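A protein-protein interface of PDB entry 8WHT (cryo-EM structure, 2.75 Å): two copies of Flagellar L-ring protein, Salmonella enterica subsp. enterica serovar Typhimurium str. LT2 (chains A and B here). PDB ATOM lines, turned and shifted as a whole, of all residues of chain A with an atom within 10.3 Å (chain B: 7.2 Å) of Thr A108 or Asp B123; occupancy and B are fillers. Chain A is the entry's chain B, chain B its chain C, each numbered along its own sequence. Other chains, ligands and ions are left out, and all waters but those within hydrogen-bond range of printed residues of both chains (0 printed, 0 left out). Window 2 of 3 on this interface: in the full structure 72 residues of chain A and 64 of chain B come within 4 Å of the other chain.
The backbone carbonyl oxygen (O) of Glu B125 lies within hydrogen-bond range of the backbone NH (N) of Asp A107, 2.9 Å away.
The backbone NH (N) of Glu B125 sits at hydrogen-bond distance from the backbone carbonyl oxygen (O) of Thr A108 (2.7 Å).
The backbone NH (N) of Arg A111 lies within hydrogen-bond range of the backbone carbonyl oxygen (O) of Arg B121, 3.0 Å away.
N of Phe A106 sits at hydrogen-bond distance from OD1 of Asp A123, at 3.2 Å.
O of Val A109 is in hydrogen-bond range of NE2 of Gln A114.
The backbone NH (N) of Ala B126 sits at hydrogen-bond distance from the backbone carbonyl oxygen (O) of Thr B102.
The backbone NH (N) of Phe B104 sits at hydrogen-bond distance from the backbone carbonyl oxygen (O) of Met B124 (2.9 Å).
N of Phe B106 is in hydrogen-bond range of OD1 of Asp B123, 3.2 Å away.
The backbone carbonyl oxygen of Gly B118 lies close to the guanidinium group of Arg B121, 3.3 Å away.
Among the printed residues, pairs that only touch across the chains: Gly A105 with Ala B126 (3.5 Å), Phe A106 with Glu B125 (3.3 Å), Phe A106 with Ala B126 (3.9 Å), Thr A108 with Asp B123 (3.5 Å), Thr A108 with Met B124 (3.2 Å), Val A109 with Asp B123 (3.97 Å), Pro A110 with Arg B121 (3.7 Å), Pro A110 with Asp B123 (3.7 Å) and Pro A110 with Met B124 (3.0 Å).
Of the printed residues of chain B, Phe A106 touches Glu B125 and Ala B126.
Printed residues of chain B within 4 Å of Asp A107: Glu B125 (2.9 Å).
Printed residues of chain B within 4 Å of Val A109: Asp B123.
Of the printed residues of chain B, Arg A111 touches Arg B121.
No residue of chain A comes within 4 Å of Ser B120.
Of the printed residues of chain A, Arg B121 touches Pro A110 and Arg A111.
No residue of chain A comes within 4 Å of Ala B122.
Of chain A, only Thr A108, Val A109 and Pro A110 come within 4 Å of Asp B123.
Of chain A, only Phe A106 (3.3 Å), Asp A107 (2.9 Å) and Thr A108 (2.7 Å) come within 4 Å of Glu B125.
Of the 16 printed residues of chain A, 7 touch a printed residue of chain B.
Printed residues of chain A that touch a printed residue of chain B: Gly A105, Phe A106, Asp A107, Thr A108, Val A109, Pro A110 and Arg A111.
Hydrophobic or aromatic side chains of chain A within 4 Å of the printed part of chain B: Phe A106 and Pro A110.
Of the 17 printed residues of chain B, 5 touch a printed residue of chain A.
Along chain B the printed residues that touch a printed residue of chain A span positions 121 to 126.
Among the printed residues, no Asp or Glu carboxylate lies within 4 Å of a Lys or Arg side-chain nitrogen of the other chain.
Val A109 touches Asp B123, but with the chains exchanged Asp A123 does not touch Val B109 (23.7 Å).
Positions printed for both chains: 104, 105, 106, 107, 109, 117, 118, 119, 120 and 123.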
ATOM      1  N   PHE A 104      -8.930  24.535   3.901  1.00  0.00           N
ATOM      2  CA  PHE A 104     -10.351  24.843   3.949  1.00  0.00           C
ATOM      3  C   PHE A 104     -10.877  24.446   5.318  1.00  0.00           C
ATOM      4  O   PHE A 104     -10.635  23.326   5.775  1.00  0.00           O
ATOM      5  CB  PHE A 104     -11.133  24.115   2.855  1.00  0.00           C
ATOM      6  CG  PHE A 104     -12.622  24.279   2.974  1.00  0.00           C
ATOM      7  CD1 PHE A 104     -13.215  25.515   2.774  1.00  0.00           C
ATOM      8  CD2 PHE A 104     -13.427  23.203   3.307  1.00  0.00           C
ATOM      9  CE1 PHE A 104     -14.580  25.671   2.891  1.00  0.00           C
ATOM     10  CE2 PHE A 104     -14.795  23.356   3.426  1.00  0.00           C
ATOM     11  CZ  PHE A 104     -15.371  24.591   3.218  1.00  0.00           C
ATOM     12  N   GLY A 105     -11.591  25.363   5.962  1.00  0.00           N
ATOM     13  CA  GLY A 105     -12.157  25.093   7.265  1.00  0.00           C
ATOM     14  C   GLY A 105     -13.542  25.675   7.451  1.00  0.00           C
ATOM     15  O   GLY A 105     -13.806  26.810   7.048  1.00  0.00           O
ATOM     16  N   PHE A 106     -14.432  24.903   8.062  1.00  0.00           N
ATOM     17  CA  PHE A 106     -15.785  25.342   8.392  1.00  0.00           C
ATOM     18  C   PHE A 106     -15.844  25.502   9.909  1.00  0.00           C
ATOM     19  O   PHE A 106     -16.043  24.534  10.643  1.00  0.00           O
ATOM     20  CB  PHE A 106     -16.821  24.346   7.884  1.00  0.00           C
ATOM     21  CG  PHE A 106     -17.926  24.972   7.083  1.00  0.00           C
ATOM     22  CD1 PHE A 106     -18.721  25.963   7.627  1.00  0.00           C
ATOM     23  CD2 PHE A 106     -18.175  24.559   5.785  1.00  0.00           C
ATOM     24  CE1 PHE A 106     -19.741  26.537   6.891  1.00  0.00           C
ATOM     25  CE2 PHE A 106     -19.193  25.129   5.045  1.00  0.00           C
ATOM     26  CZ  PHE A 106     -19.976  26.119   5.600  1.00  0.00           C
ATOM     27  N   ASP A 107     -15.655  26.737  10.376  1.00  0.00           N
ATOM     28  CA  ASP A 107     -15.646  26.993  11.814  1.00  0.00           C
ATOM     29  C   ASP A 107     -17.038  26.823  12.410  1.00  0.00           C
ATOM     30  O   ASP A 107     -17.210  26.145  13.430  1.00  0.00           O
ATOM     31  CB  ASP A 107     -15.109  28.396  12.089  1.00  0.00           C
ATOM     32  CG  ASP A 107     -13.648  28.543  11.711  1.00  0.00           C
ATOM     33  OD1 ASP A 107     -12.804  27.838  12.302  1.00  0.00           O
ATOM     34  OD2 ASP A 107     -13.346  29.364  10.820  1.00  0.00           O
ATOM     35  N   THR A 108     -18.042  27.432  11.787  1.00  0.00           N
ATOM     36  CA  THR A 108     -19.434  27.303  12.199  1.00  0.00           C
ATOM     37  C   THR A 108     -20.236  26.805  11.008  1.00  0.00           C
ATOM     38  O   THR A 108     -20.241  27.443   9.950  1.00  0.00           O
ATOM     39  CB  THR A 108     -19.992  28.636  12.703  1.00  0.00           C
ATOM     40  OG1 THR A 108     -19.065  29.230  13.620  1.00  0.00           O
ATOM     41  CG2 THR A 108     -21.323  28.426  13.404  1.00  0.00           C
ATOM     42  N   VAL A 109     -20.908  25.676  11.177  1.00  0.00           N
ATOM     43  CA  VAL A 109     -21.667  25.032  10.110  1.00  0.00           C
ATOM     44  C   VAL A 109     -23.150  25.234  10.397  1.00  0.00           C
ATOM     45  O   VAL A 109     -23.627  24.834  11.469  1.00  0.00           O
ATOM     46  CB  VAL A 109     -21.327  23.539   9.990  1.00  0.00           C
ATOM     47  CG1 VAL A 109     -21.947  22.958   8.732  1.00  0.00           C
ATOM     48  CG2 VAL A 109     -19.821  23.341   9.990  1.00  0.00           C
ATOM     49  N   PRO A 110     -23.910  25.844   9.493  1.00  0.00           N
ATOM     50  CA  PRO A 110     -25.359  25.940   9.688  1.00  0.00           C
ATOM     51  C   PRO A 110     -26.007  24.566   9.640  1.00  0.00           C
ATOM     52  O   PRO A 110     -25.443  23.599   9.122  1.00  0.00           O
ATOM     53  CB  PRO A 110     -25.822  26.820   8.525  1.00  0.00           C
ATOM     54  CG  PRO A 110     -24.767  26.660   7.487  1.00  0.00           C
ATOM     55  CD  PRO A 110     -23.478  26.452   8.223  1.00  0.00           C
ATOM     56  N   ARG A 111     -27.212  24.489  10.209  1.00  0.00           N
ATOM     57  CA  ARG A 111     -27.869  23.196  10.376  1.00  0.00           C
ATOM     58  C   ARG A 111     -28.109  22.509   9.038  1.00  0.00           C
ATOM     59  O   ARG A 111     -27.801  21.321   8.881  1.00  0.00           O
ATOM     60  CB  ARG A 111     -29.184  23.371  11.132  1.00  0.00           C
ATOM     61  CG  ARG A 111     -29.663  22.107  11.821  1.00  0.00           C
ATOM     62  CD  ARG A 111     -30.737  22.408  12.849  1.00  0.00           C
ATOM     63  NE  ARG A 111     -31.118  21.217  13.596  1.00  0.00           N
ATOM     64  CZ  ARG A 111     -31.907  21.222  14.662  1.00  0.00           C
ATOM     65  NH1 ARG A 111     -32.418  22.345  15.139  1.00  0.00           N
ATOM     66  NH2 ARG A 111     -32.188  20.071  15.267  1.00  0.00           N
ATOM     67  N   TYR A 112     -28.629  23.242   8.053  1.00  0.00           N
ATOM     68  CA  TYR A 112     -28.939  22.644   6.759  1.00  0.00           C
ATOM     69  C   TYR A 112     -27.696  22.172   6.016  1.00  0.00           C
ATOM     70  O   TYR A 112     -27.825  21.424   5.042  1.00  0.00           O
ATOM     71  CB  TYR A 112     -29.718  23.635   5.888  1.00  0.00           C
ATOM     72  CG  TYR A 112     -28.991  24.930   5.606  1.00  0.00           C
ATOM     73  CD1 TYR A 112     -29.088  26.009   6.474  1.00  0.00           C
ATOM     74  CD2 TYR A 112     -28.214  25.077   4.465  1.00  0.00           C
ATOM     75  CE1 TYR A 112     -28.427  27.195   6.216  1.00  0.00           C
ATOM     76  CE2 TYR A 112     -27.549  26.258   4.201  1.00  0.00           C
ATOM     77  CZ  TYR A 112     -27.659  27.313   5.079  1.00  0.00           C
ATOM     78  OH  TYR A 112     -26.998  28.490   4.816  1.00  0.00           O
ATOM     79  N   LEU A 113     -26.507  22.585   6.448  1.00  0.00           N
ATOM     80  CA  LEU A 113     -25.254  22.132   5.862  1.00  0.00           C
ATOM     81  C   LEU A 113     -24.557  21.081   6.715  1.00  0.00           C
ATOM     82  O   LEU A 113     -23.538  20.529   6.282  1.00  0.00           O
ATOM     83  CB  LEU A 113     -24.319  23.322   5.638  1.00  0.00           C
ATOM     84  CG  LEU A 113     -24.506  24.108   4.342  1.00  0.00           C
ATOM     85  CD1 LEU A 113     -23.402  25.136   4.181  1.00  0.00           C
ATOM     86  CD2 LEU A 113     -24.545  23.167   3.150  1.00  0.00           C
ATOM     87  N   GLN A 114     -25.093  20.777   7.902  1.00  0.00           N
ATOM     88  CA  GLN A 114     -24.397  19.896   8.839  1.00  0.00           C
ATOM     89  C   GLN A 114     -24.025  18.573   8.186  1.00  0.00           C
ATOM     90  O   GLN A 114     -22.849  18.185   8.170  1.00  0.00           O
ATOM     91  CB  GLN A 114     -25.269  19.651  10.072  1.00  0.00           C
ATOM     92  CG  GLN A 114     -25.276  20.784  11.079  1.00  0.00           C
ATOM     93  CD  GLN A 114     -24.035  20.800  11.943  1.00  0.00           C
ATOM     94  OE1 GLN A 114     -23.343  19.793  12.074  1.00  0.00           O
ATOM     95  NE2 GLN A 114     -23.750  21.949  12.547  1.00  0.00           N
ATOM     96  N   PHE A 117     -21.088  19.133   5.990  1.00  0.00           N
ATOM     97  CA  PHE A 117     -19.892  19.808   6.479  1.00  0.00           C
ATOM     98  C   PHE A 117     -19.692  19.671   7.984  1.00  0.00           C
ATOM     99  O   PHE A 117     -18.719  20.215   8.516  1.00  0.00           O
ATOM    100  CB  PHE A 117     -19.919  21.293   6.092  1.00  0.00           C
ATOM    101  CG  PHE A 117     -19.777  21.536   4.616  1.00  0.00           C
ATOM    102  CD1 PHE A 117     -18.556  21.357   3.988  1.00  0.00           C
ATOM    103  CD2 PHE A 117     -20.860  21.944   3.857  1.00  0.00           C
ATOM    104  CE1 PHE A 117     -18.421  21.578   2.632  1.00  0.00           C
ATOM    105  CE2 PHE A 117     -20.730  22.167   2.501  1.00  0.00           C
ATOM    106  CZ  PHE A 117     -19.507  21.984   1.888  1.00  0.00           C
ATOM    107  N   GLY A 118     -20.578  18.963   8.682  1.00  0.00           N
ATOM    108  CA  GLY A 118     -20.416  18.767  10.105  1.00  0.00           C
ATOM    109  C   GLY A 118     -19.338  17.755  10.435  1.00  0.00           C
ATOM    110  O   GLY A 118     -18.900  16.983   9.585  1.00  0.00           O
ATOM    111  N   ASN A 119     -18.913  17.778  11.699  1.00  0.00           N
ATOM    112  CA  ASN A 119     -17.882  16.874  12.212  1.00  0.00           C
ATOM    113  C   ASN A 119     -16.579  16.997  11.426  1.00  0.00           C
ATOM    114  O   ASN A 119     -15.836  16.021  11.285  1.00  0.00           O
ATOM    115  CB  ASN A 119     -18.374  15.422  12.219  1.00  0.00           C
ATOM    116  CG  ASN A 119     -17.704  14.582  13.289  1.00  0.00           C
ATOM    117  OD1 ASN A 119     -16.943  13.663  12.988  1.00  0.00           O
ATOM    118  ND2 ASN A 119     -17.987  14.893  14.548  1.00  0.00           N
ATOM    119  N   SER A 120     -16.292  18.202  10.927  1.00  0.00           N
ATOM    120  CA  SER A 120     -15.081  18.492  10.149  1.00  0.00           C
ATOM    121  C   SER A 120     -14.890  17.489   9.015  1.00  0.00           C
ATOM    122  O   SER A 120     -13.787  16.990   8.773  1.00  0.00           O
ATOM    123  CB  SER A 120     -13.840  18.548  11.046  1.00  0.00           C
ATOM    124  OG  SER A 120     -13.781  17.457  11.948  1.00  0.00           O
ATOM    125  N   ASP A 123     -13.171  19.728   6.258  1.00  0.00           N
ATOM    126  CA  ASP A 123     -12.009  20.504   6.677  1.00  0.00           C
ATOM    127  C   ASP A 123     -10.728  19.786   6.276  1.00  0.00           C
ATOM    128  O   ASP A 123     -10.577  18.584   6.510  1.00  0.00           O
ATOM    129  CB  ASP A 123     -12.037  20.725   8.189  1.00  0.00           C
ATOM    130  CG  ASP A 123     -13.178  21.623   8.628  1.00  0.00           C
ATOM    131  OD1 ASP A 123     -14.199  21.689   7.911  1.00  0.00           O
ATOM    132  OD2 ASP A 123     -13.054  22.265   9.692  1.00  0.00           O
ATOM    133  N   THR B 102     -16.098  33.918   4.808  1.00  0.00           N
ATOM    134  CA  THR B 102     -17.525  34.200   4.807  1.00  0.00           C
ATOM    135  C   THR B 102     -18.080  33.916   6.194  1.00  0.00           C
ATOM    136  O   THR B 102     -17.636  32.991   6.876  1.00  0.00           O
ATOM    137  CB  THR B 102     -18.273  33.361   3.762  1.00  0.00           C
ATOM    138  OG1 THR B 102     -17.454  33.202   2.599  1.00  0.00           O
ATOM    139  CG2 THR B 102     -19.562  34.053   3.354  1.00  0.00           C
ATOM    140  N   SER B 103     -19.050  34.726   6.611  1.00  0.00           N
ATOM    141  CA  SER B 103     -19.647  34.559   7.925  1.00  0.00           C
ATOM    142  C   SER B 103     -21.055  35.132   7.926  1.00  0.00           C
ATOM    143  O   SER B 103     -21.390  36.006   7.122  1.00  0.00           O
ATOM    144  CB  SER B 103     -18.805  35.234   9.013  1.00  0.00           C
ATOM    145  OG  SER B 103     -19.349  36.492   9.369  1.00  0.00           O
ATOM    146  N   PHE B 104     -21.877  34.618   8.837  1.00  0.00           N
ATOM    147  CA  PHE B 104     -23.195  35.171   9.111  1.00  0.00           C
ATOM    148  C   PHE B 104     -23.582  34.793  10.530  1.00  0.00           C
ATOM    149  O   PHE B 104     -23.489  33.622  10.908  1.00  0.00           O
ATOM    150  CB  PHE B 104     -24.249  34.661   8.126  1.00  0.00           C
ATOM    151  CG  PHE B 104     -25.648  35.081   8.477  1.00  0.00           C
ATOM    152  CD1 PHE B 104     -26.024  36.412   8.409  1.00  0.00           C
ATOM    153  CD2 PHE B 104     -26.582  34.148   8.894  1.00  0.00           C
ATOM    154  CE1 PHE B 104     -27.306  36.803   8.739  1.00  0.00           C
ATOM    155  CE2 PHE B 104     -27.866  34.535   9.225  1.00  0.00           C
ATOM    156  CZ  PHE B 104     -28.227  35.863   9.147  1.00  0.00           C
ATOM    157  N   GLY B 105     -24.013  35.783  11.306  1.00  0.00           N
ATOM    158  CA  GLY B 105     -24.427  35.540  12.671  1.00  0.00           C
ATOM    159  C   GLY B 105     -25.638  36.348  13.084  1.00  0.00           C
ATOM    160  O   GLY B 105     -25.743  37.534  12.763  1.00  0.00           O
ATOM    161  N   PHE B 106     -26.558  35.712  13.799  1.00  0.00           N
ATOM    162  CA  PHE B 106     -27.744  36.365  14.346  1.00  0.00           C
ATOM    163  C   PHE B 106     -27.553  36.441  15.859  1.00  0.00           C
ATOM    164  O   PHE B 106     -27.822  35.482  16.582  1.00  0.00           O
ATOM    165  CB  PHE B 106     -29.010  35.602  13.970  1.00  0.00           C
ATOM    166  CG  PHE B 106     -30.083  36.462  13.367  1.00  0.00           C
ATOM    167  CD1 PHE B 106     -30.593  37.544  14.059  1.00  0.00           C
ATOM    168  CD2 PHE B 106     -30.588  36.179  12.111  1.00  0.00           C
ATOM    169  CE1 PHE B 106     -31.584  38.334  13.507  1.00  0.00           C
ATOM    170  CE2 PHE B 106     -31.579  36.964  11.554  1.00  0.00           C
ATOM    171  CZ  PHE B 106     -32.076  38.042  12.253  1.00  0.00           C
ATOM    172  N   ASP B 107     -27.072  37.593  16.332  1.00  0.00           N
ATOM    173  CA  ASP B 107     -26.810  37.755  17.758  1.00  0.00           C
ATOM    174  C   ASP B 107     -28.108  37.802  18.555  1.00  0.00           C
ATOM    175  O   ASP B 107     -28.255  37.105  19.565  1.00  0.00           O
ATOM    176  CB  ASP B 107     -25.987  39.022  17.993  1.00  0.00           C
ATOM    177  CG  ASP B 107     -24.595  38.928  17.402  1.00  0.00           C
ATOM    178  OD1 ASP B 107     -23.820  38.049  17.834  1.00  0.00           O
ATOM    179  OD2 ASP B 107     -24.277  39.734  16.502  1.00  0.00           O
ATOM    180  N   VAL B 109     -32.261  37.440  17.890  1.00  0.00           N
ATOM    181  CA  VAL B 109     -33.272  37.008  16.931  1.00  0.00           C
ATOM    182  C   VAL B 109     -34.634  37.453  17.448  1.00  0.00           C
ATOM    183  O   VAL B 109     -35.018  37.080  18.566  1.00  0.00           O
ATOM    184  CB  VAL B 109     -33.235  35.488  16.712  1.00  0.00           C
ATOM    185  CG1 VAL B 109     -34.127  35.101  15.545  1.00  0.00           C
ATOM    186  CG2 VAL B 109     -31.808  35.023  16.475  1.00  0.00           C
ATOM    187  N   PHE B 117     -34.396  31.357  12.581  1.00  0.00           N
ATOM    188  CA  PHE B 117     -33.038  31.777  12.904  1.00  0.00           C
ATOM    189  C   PHE B 117     -32.653  31.517  14.355  1.00  0.00           C
ATOM    190  O   PHE B 117     -31.529  31.846  14.750  1.00  0.00           O
ATOM    191  CB  PHE B 117     -32.845  33.263  12.574  1.00  0.00           C
ATOM    192  CG  PHE B 117     -32.875  33.566  11.101  1.00  0.00           C
ATOM    193  CD1 PHE B 117     -31.812  33.209  10.289  1.00  0.00           C
ATOM    194  CD2 PHE B 117     -33.961  34.205  10.531  1.00  0.00           C
ATOM    195  CE1 PHE B 117     -31.834  33.483   8.936  1.00  0.00           C
ATOM    196  CE2 PHE B 117     -33.989  34.482   9.178  1.00  0.00           C
ATOM    197  CZ  PHE B 117     -32.923  34.121   8.381  1.00  0.00           C
ATOM    198  N   GLY B 118     -33.544  30.937  15.156  1.00  0.00           N
ATOM    199  CA  GLY B 118     -33.219  30.631  16.531  1.00  0.00           C
ATOM    200  C   GLY B 118     -32.310  29.425  16.659  1.00  0.00           C
ATOM    201  O   GLY B 118     -32.150  28.640  15.727  1.00  0.00           O
ATOM    202  N   ASN B 119     -31.711  29.296  17.844  1.00  0.00           N
ATOM    203  CA  ASN B 119     -30.802  28.193  18.163  1.00  0.00           C
ATOM    204  C   ASN B 119     -29.625  28.128  17.192  1.00  0.00           C
ATOM    205  O   ASN B 119     -29.105  27.046  16.907  1.00  0.00           O
ATOM    206  CB  ASN B 119     -31.548  26.854  18.198  1.00  0.00           C
ATOM    207  CG  ASN B 119     -30.899  25.845  19.125  1.00  0.00           C
ATOM    208  OD1 ASN B 119     -30.373  24.826  18.682  1.00  0.00           O
ATOM    209  ND2 ASN B 119     -30.934  26.127  20.423  1.00  0.00           N
ATOM    210  N   SER B 120     -29.195  29.291  16.695  1.00  0.00           N
ATOM    211  CA  SER B 120     -28.076  29.406  15.751  1.00  0.00           C
ATOM    212  C   SER B 120     -28.240  28.455  14.569  1.00  0.00           C
ATOM    213  O   SER B 120     -27.297  27.783  14.145  1.00  0.00           O
ATOM    214  CB  SER B 120     -26.730  29.185  16.449  1.00  0.00           C
ATOM    215  OG  SER B 120     -26.745  28.050  17.295  1.00  0.00           O
ATOM    216  N   ARG B 121     -29.458  28.399  14.025  1.00  0.00           N
ATOM    217  CA  ARG B 121     -29.735  27.473  12.932  1.00  0.00           C
ATOM    218  C   ARG B 121     -29.089  27.923  11.628  1.00  0.00           C
ATOM    219  O   ARG B 121     -28.704  27.080  10.808  1.00  0.00           O
ATOM    220  CB  ARG B 121     -31.244  27.313  12.751  1.00  0.00           C
ATOM    221  CG  ARG B 121     -31.857  26.247  13.642  1.00  0.00           C
ATOM    222  CD  ARG B 121     -33.288  25.937  13.239  1.00  0.00           C
ATOM    223  NE  ARG B 121     -34.241  26.837  13.877  1.00  0.00           N
ATOM    224  CZ  ARG B 121     -34.871  26.576  15.014  1.00  0.00           C
ATOM    225  NH1 ARG B 121     -34.666  25.448  15.676  1.00  0.00           N
ATOM    226  NH2 ARG B 121     -35.731  27.468  15.500  1.00  0.00           N
ATOM    227  N   ALA B 122     -28.963  29.230  11.413  1.00  0.00           N
ATOM    228  CA  ALA B 122     -28.373  29.761  10.192  1.00  0.00           C
ATOM    229  C   ALA B 122     -27.006  30.392  10.409  1.00  0.00           C
ATOM    230  O   ALA B 122     -26.362  30.783   9.432  1.00  0.00           O
ATOM    231  CB  ALA B 122     -29.318  30.784   9.552  1.00  0.00           C
ATOM    232  N   ASP B 123     -26.552  30.512  11.656  1.00  0.00           N
ATOM    233  CA  ASP B 123     -25.219  31.042  11.918  1.00  0.00           C
ATOM    234  C   ASP B 123     -24.165  30.132  11.302  1.00  0.00           C
ATOM    235  O   ASP B 123     -24.206  28.911  11.472  1.00  0.00           O
ATOM    236  CB  ASP B 123     -24.986  31.174  13.423  1.00  0.00           C
ATOM    237  CG  ASP B 123     -25.866  32.232  14.060  1.00  0.00           C
ATOM    238  OD1 ASP B 123     -26.948  32.522  13.509  1.00  0.00           O
ATOM    239  OD2 ASP B 123     -25.474  32.777  15.112  1.00  0.00           O
ATOM    240  N   MET B 124     -23.212  30.729  10.588  1.00  0.00           N
ATOM    241  CA  MET B 124     -22.197  29.942   9.903  1.00  0.00           C
ATOM    242  C   MET B 124     -20.955  30.792   9.690  1.00  0.00           C
ATOM    243  O   MET B 124     -20.998  32.022   9.756  1.00  0.00           O
ATOM    244  CB  MET B 124     -22.745  29.372   8.583  1.00  0.00           C
ATOM    245  CG  MET B 124     -22.651  30.270   7.352  1.00  0.00           C
ATOM    246  SD  MET B 124     -21.042  30.335   6.540  1.00  0.00           S
ATOM    247  CE  MET B 124     -21.131  31.955   5.791  1.00  0.00           C
ATOM    248  N   GLU B 125     -19.839  30.112   9.439  1.00  0.00           N
ATOM    249  CA  GLU B 125     -18.551  30.771   9.247  1.00  0.00           C
ATOM    250  C   GLU B 125     -17.616  29.801   8.546  1.00  0.00           C
ATOM    251  O   GLU B 125     -17.398  28.691   9.040  1.00  0.00           O
ATOM    252  CB  GLU B 125     -17.962  31.218  10.583  1.00  0.00           C
ATOM    253  CG  GLU B 125     -16.698  32.046  10.464  1.00  0.00           C
ATOM    254  CD  GLU B 125     -16.022  32.262  11.802  1.00  0.00           C
ATOM    255  OE1 GLU B 125     -16.271  31.464  12.730  1.00  0.00           O
ATOM    256  OE2 GLU B 125     -15.238  33.226  11.927  1.00  0.00           O
ATOM    257  N   ALA B 126     -17.070  30.209   7.404  1.00  0.00           N
ATOM    258  CA  ALA B 126     -16.156  29.380   6.637  1.00  0.00           C
ATOM    259  C   ALA B 126     -14.981  30.211   6.144  1.00  0.00           C
ATOM    260  O   ALA B 126     -15.087  31.427   5.958  1.00  0.00           O
ATOM    261  CB  ALA B 126     -16.860  28.717   5.447  1.00  0.00           C
